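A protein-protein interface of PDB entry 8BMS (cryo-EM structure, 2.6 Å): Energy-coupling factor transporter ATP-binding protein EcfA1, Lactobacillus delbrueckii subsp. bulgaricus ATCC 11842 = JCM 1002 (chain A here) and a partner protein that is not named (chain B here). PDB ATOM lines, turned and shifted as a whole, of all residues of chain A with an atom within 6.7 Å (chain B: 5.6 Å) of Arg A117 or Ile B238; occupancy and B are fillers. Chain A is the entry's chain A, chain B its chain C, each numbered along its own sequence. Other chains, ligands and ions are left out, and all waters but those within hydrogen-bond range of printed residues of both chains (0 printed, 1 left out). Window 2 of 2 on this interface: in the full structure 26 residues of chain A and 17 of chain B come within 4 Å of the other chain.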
ATOM      1  N   ALA A 114     -12.543  -3.875 -27.342  1.00  0.00           N
ATOM      2  CA  ALA A 114     -13.185  -3.087 -26.288  1.00  0.00           C
ATOM      3  C   ALA A 114     -12.563  -3.360 -24.920  1.00  0.00           C
ATOM      4  O   ALA A 114     -13.255  -3.420 -23.903  1.00  0.00           O
ATOM      5  CB  ALA A 114     -14.695  -3.330 -26.255  1.00  0.00           C
ATOM      6  N   VAL A 115     -11.249  -3.532 -24.897  1.00  0.00           N
ATOM      7  CA  VAL A 115     -10.536  -3.659 -23.621  1.00  0.00           C
ATOM      8  C   VAL A 115     -10.439  -2.282 -22.972  1.00  0.00           C
ATOM      9  O   VAL A 115     -10.080  -1.307 -23.654  1.00  0.00           O
ATOM     10  CB  VAL A 115      -9.148  -4.265 -23.845  1.00  0.00           C
ATOM     11  CG1 VAL A 115      -8.367  -4.311 -22.542  1.00  0.00           C
ATOM     12  CG2 VAL A 115      -9.269  -5.656 -24.440  1.00  0.00           C
ATOM     13  N   PRO A 116     -10.771  -2.141 -21.688  1.00  0.00           N
ATOM     14  CA  PRO A 116     -10.688  -0.821 -21.049  1.00  0.00           C
ATOM     15  C   PRO A 116      -9.269  -0.273 -21.068  1.00  0.00           C
ATOM     16  O   PRO A 116      -8.293  -1.014 -20.938  1.00  0.00           O
ATOM     17  CB  PRO A 116     -11.175  -1.085 -19.618  1.00  0.00           C
ATOM     18  CG  PRO A 116     -11.098  -2.563 -19.438  1.00  0.00           C
ATOM     19  CD  PRO A 116     -11.329  -3.158 -20.785  1.00  0.00           C
ATOM     20  N   ARG A 117      -9.169   1.047 -21.227  1.00  0.00           N
ATOM     21  CA  ARG A 117      -7.865   1.693 -21.346  1.00  0.00           C
ATOM     22  C   ARG A 117      -6.942   1.463 -20.152  1.00  0.00           C
ATOM     23  O   ARG A 117      -5.735   1.263 -20.380  1.00  0.00           O
ATOM     24  CB  ARG A 117      -8.058   3.193 -21.599  1.00  0.00           C
ATOM     25  CG  ARG A 117      -6.791   3.918 -22.011  1.00  0.00           C
ATOM     26  CD  ARG A 117      -7.002   5.419 -22.048  1.00  0.00           C
ATOM     27  NE  ARG A 117      -5.756   6.146 -21.837  1.00  0.00           N
ATOM     28  CZ  ARG A 117      -5.241   6.415 -20.645  1.00  0.00           C
ATOM     29  NH1 ARG A 117      -5.837   6.027 -19.531  1.00  0.00           N
ATOM     30  NH2 ARG A 117      -4.098   7.091 -20.571  1.00  0.00           N
ATOM     31  N   PRO A 118      -7.399   1.512 -18.892  1.00  0.00           N
ATOM     32  CA  PRO A 118      -6.472   1.206 -17.787  1.00  0.00           C
ATOM     33  C   PRO A 118      -5.823  -0.162 -17.904  1.00  0.00           C
ATOM     34  O   PRO A 118      -4.646  -0.315 -17.556  1.00  0.00           O
ATOM     35  CB  PRO A 118      -7.369   1.307 -16.546  1.00  0.00           C
ATOM     36  CG  PRO A 118      -8.421   2.265 -16.934  1.00  0.00           C
ATOM     37  CD  PRO A 118      -8.694   2.004 -18.385  1.00  0.00           C
ATOM     38  N   GLU A 119      -6.559  -1.166 -18.385  1.00  0.00           N
ATOM     39  CA  GLU A 119      -5.954  -2.468 -18.631  1.00  0.00           C
ATOM     40  C   GLU A 119      -5.102  -2.468 -19.893  1.00  0.00           C
ATOM     41  O   GLU A 119      -4.082  -3.165 -19.944  1.00  0.00           O
ATOM     42  CB  GLU A 119      -7.034  -3.545 -18.728  1.00  0.00           C
ATOM     43  CG  GLU A 119      -7.934  -3.632 -17.510  1.00  0.00           C
ATOM     44  CD  GLU A 119      -9.026  -4.670 -17.668  1.00  0.00           C
ATOM     45  OE1 GLU A 119      -8.868  -5.575 -18.513  1.00  0.00           O
ATOM     46  OE2 GLU A 119     -10.043  -4.580 -16.948  1.00  0.00           O
ATOM     47  N   MET A 120      -5.504  -1.702 -20.910  1.00  0.00           N
ATOM     48  CA  MET A 120      -4.726  -1.634 -22.142  1.00  0.00           C
ATOM     49  C   MET A 120      -3.333  -1.081 -21.893  1.00  0.00           C
ATOM     50  O   MET A 120      -2.366  -1.535 -22.506  1.00  0.00           O
ATOM     51  CB  MET A 120      -5.433  -0.780 -23.188  1.00  0.00           C
ATOM     52  CG  MET A 120      -6.721  -1.343 -23.717  1.00  0.00           C
ATOM     53  SD  MET A 120      -7.424  -0.158 -24.864  1.00  0.00           S
ATOM     54  CE  MET A 120      -6.239  -0.334 -26.185  1.00  0.00           C
ATOM     55  N   LEU A 121      -3.214  -0.072 -21.029  1.00  0.00           N
ATOM     56  CA  LEU A 121      -1.897   0.492 -20.750  1.00  0.00           C
ATOM     57  C   LEU A 121      -0.944  -0.585 -20.245  1.00  0.00           C
ATOM     58  O   LEU A 121       0.160  -0.761 -20.780  1.00  0.00           O
ATOM     59  CB  LEU A 121      -2.016   1.628 -19.733  1.00  0.00           C
ATOM     60  CG  LEU A 121      -2.887   2.822 -20.124  1.00  0.00           C
ATOM     61  CD1 LEU A 121      -2.972   3.818 -18.981  1.00  0.00           C
ATOM     62  CD2 LEU A 121      -2.359   3.488 -21.381  1.00  0.00           C
ATOM     63  N   LYS A 122      -1.375  -1.339 -19.231  1.00  0.00           N
ATOM     64  CA  LYS A 122      -0.541  -2.398 -18.677  1.00  0.00           C
ATOM     65  C   LYS A 122      -0.267  -3.488 -19.703  1.00  0.00           C
ATOM     66  O   LYS A 122       0.864  -3.974 -19.812  1.00  0.00           O
ATOM     67  CB  LYS A 122      -1.206  -2.992 -17.436  1.00  0.00           C
ATOM     68  CG  LYS A 122      -1.503  -1.981 -16.347  1.00  0.00           C
ATOM     69  CD  LYS A 122      -1.895  -2.674 -15.055  1.00  0.00           C
ATOM     70  CE  LYS A 122      -3.115  -3.557 -15.251  1.00  0.00           C
ATOM     71  NZ  LYS A 122      -3.483  -4.284 -14.006  1.00  0.00           N
ATOM     72  N   THR B 234     -12.542   0.886 -27.900  1.00  0.00           N
ATOM     73  CA  THR B 234     -11.973   1.752 -26.884  1.00  0.00           C
ATOM     74  C   THR B 234     -10.799   2.520 -27.485  1.00  0.00           C
ATOM     75  O   THR B 234     -10.436   2.340 -28.650  1.00  0.00           O
ATOM     76  CB  THR B 234     -11.547   0.946 -25.656  1.00  0.00           C
ATOM     77  OG1 THR B 234     -10.812  -0.211 -26.068  1.00  0.00           O
ATOM     78  CG2 THR B 234     -12.766   0.510 -24.859  1.00  0.00           C
ATOM     79  N   ARG B 235     -10.198   3.394 -26.684  1.00  0.00           N
ATOM     80  CA  ARG B 235      -9.135   4.268 -27.159  1.00  0.00           C
ATOM     81  C   ARG B 235      -7.902   4.108 -26.286  1.00  0.00           C
ATOM     82  O   ARG B 235      -7.994   4.167 -25.057  1.00  0.00           O
ATOM     83  CB  ARG B 235      -9.588   5.731 -27.164  1.00  0.00           C
ATOM     84  CG  ARG B 235     -10.364   6.137 -28.403  1.00  0.00           C
ATOM     85  CD  ARG B 235     -10.320   7.641 -28.608  1.00  0.00           C
ATOM     86  NE  ARG B 235      -8.955   8.135 -28.737  1.00  0.00           N
ATOM     87  CZ  ARG B 235      -8.521   8.886 -29.740  1.00  0.00           C
ATOM     88  NH1 ARG B 235      -9.321   9.252 -30.727  1.00  0.00           N
ATOM     89  NH2 ARG B 235      -7.251   9.283 -29.752  1.00  0.00           N
ATOM     90  N   TYR B 236      -6.749   3.903 -26.927  1.00  0.00           N
ATOM     91  CA  TYR B 236      -5.484   3.921 -26.202  1.00  0.00           C
ATOM     92  C   TYR B 236      -5.127   5.335 -25.763  1.00  0.00           C
ATOM     93  O   TYR B 236      -4.582   5.535 -24.672  1.00  0.00           O
ATOM     94  CB  TYR B 236      -4.377   3.327 -27.072  1.00  0.00           C
ATOM     95  CG  TYR B 236      -3.092   3.038 -26.329  1.00  0.00           C
ATOM     96  CD1 TYR B 236      -3.083   2.207 -25.220  1.00  0.00           C
ATOM     97  CD2 TYR B 236      -1.890   3.595 -26.742  1.00  0.00           C
ATOM     98  CE1 TYR B 236      -1.912   1.940 -24.539  1.00  0.00           C
ATOM     99  CE2 TYR B 236      -0.716   3.335 -26.068  1.00  0.00           C
ATOM    100  CZ  TYR B 236      -0.732   2.508 -24.967  1.00  0.00           C
ATOM    101  OH  TYR B 236       0.435   2.244 -24.291  1.00  0.00           O
ATOM    102  N   ARG B 237      -5.428   6.323 -26.599  1.00  0.00           N
ATOM    103  CA  ARG B 237      -5.166   7.722 -26.303  1.00  0.00           C
ATOM    104  C   ARG B 237      -6.463   8.421 -25.917  1.00  0.00           C
ATOM    105  O   ARG B 237      -7.497   8.232 -26.563  1.00  0.00           O
ATOM    106  CB  ARG B 237      -4.531   8.423 -27.505  1.00  0.00           C
ATOM    107  CG  ARG B 237      -3.409   7.639 -28.165  1.00  0.00           C
ATOM    108  CD  ARG B 237      -2.159   7.617 -27.299  1.00  0.00           C
ATOM    109  NE  ARG B 237      -1.031   7.006 -27.991  1.00  0.00           N
ATOM    110  CZ  ARG B 237       0.198   6.928 -27.499  1.00  0.00           C
ATOM    111  NH1 ARG B 237       0.498   7.414 -26.306  1.00  0.00           N
ATOM    112  NH2 ARG B 237       1.151   6.349 -28.224  1.00  0.00           N
ATOM    113  N   ILE B 238      -6.401   9.228 -24.859  1.00  0.00           N
ATOM    114  CA  ILE B 238      -7.590   9.909 -24.360  1.00  0.00           C
ATOM    115  C   ILE B 238      -8.031  10.967 -25.362  1.00  0.00           C
ATOM    116  O   ILE B 238      -7.216  11.760 -25.853  1.00  0.00           O
ATOM    117  CB  ILE B 238      -7.318  10.527 -22.982  1.00  0.00           C
ATOM    118  CG1 ILE B 238      -6.998   9.435 -21.962  1.00  0.00           C
ATOM    119  CG2 ILE B 238      -8.512  11.342 -22.516  1.00  0.00           C
ATOM    120  CD1 ILE B 238      -6.468   9.968 -20.651  1.00  0.00           C
ATOM    121  N   LEU B 239      -9.324  10.983 -25.671  1.00  0.00           N
ATOM    122  CA  LEU B 239      -9.923  11.956 -26.581  1.00  0.00           C
ATOM    123  C   LEU B 239     -10.917  12.791 -25.780  1.00  0.00           C
ATOM    124  O   LEU B 239     -12.105  12.467 -25.710  1.00  0.00           O
ATOM    125  CB  LEU B 239     -10.596  11.265 -27.764  1.00  0.00           C
ATOM    126  CG  LEU B 239     -11.140  12.186 -28.855  1.00  0.00           C
ATOM    127  CD1 LEU B 239     -10.002  12.822 -29.628  1.00  0.00           C
ATOM    128  CD2 LEU B 239     -12.066  11.422 -29.787  1.00  0.00           C
ATOM    129  N   GLU B 240     -10.426  13.869 -25.173  1.00  0.00           N
ATOM    130  CA  GLU B 240     -11.256  14.751 -24.368  1.00  0.00           C
ATOM    131  C   GLU B 240     -10.862  16.197 -24.621  1.00  0.00           C
ATOM    132  O   GLU B 240      -9.709  16.496 -24.943  1.00  0.00           O
ATOM    133  CB  GLU B 240     -11.129  14.432 -22.872  1.00  0.00           C
ATOM    134  CG  GLU B 240     -11.870  13.181 -22.434  1.00  0.00           C
ATOM    135  CD  GLU B 240     -12.248  13.215 -20.966  1.00  0.00           C
ATOM    136  OE1 GLU B 240     -11.503  13.829 -20.174  1.00  0.00           O
ATOM    137  OE2 GLU B 240     -13.288  12.627 -20.604  1.00  0.00           O
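The backbone carbonyl oxygen (O) of Val A115 sits at hydrogen-bond distance from the side-chain hydroxyl (OG1) of Thr B234 (2.8 Å).
O of Tyr B236 is in hydrogen-bond range of NE of Arg A117 (3.1 Å).
The side-chain hydroxyl (OG1) of Thr B234 lies within hydrogen-bond range of the side-chain sulfur (SD) of Met A120, 3.6 Å away.
Of chain B, only Arg B235 (3.3 Å), Tyr B236 (3.1 Å) and Ile B238 (3.5 Å) come within 4 Å of Arg A117.
Ile B238 touches one residue of chain A.
Of the printed residues of chain B, Leu A121 touches Tyr B236.
Of the printed residues of chain A, Tyr B236 touches Arg A117 (3.1 Å) and Leu A121 (3.5 Å).
Printed residues of chain B within 4 Å of Ala A114: Thr B234.
The nearest residue of chain B that does not touch Arg A117 is Arg B237 (4.7 Å).
The nearest printed residue of chain A that does not touch Ile B238 is Leu A121 (7.3 Å).
The nearest printed residue of chain A that does not touch Tyr B236 is Met A120 (4.1 Å).
Among the printed residues, pairs that only touch across the chains: Arg A117 with Arg B235, Arg A117 with Ile B238, Leu A121 with Tyr B236 and Ala A114 with Thr B234.
The backbone carbonyl oxygen (O) of Arg B237 lies within hydrogen-bond range of the guanidinium group (NE) of Arg B235.
Hydrophobic or aromatic side chains of chain A that line the printed part of chain B: Met A120 and Leu A121.
Along chain A the printed residues that touch a printed residue of chain B span positions 114 to 121.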
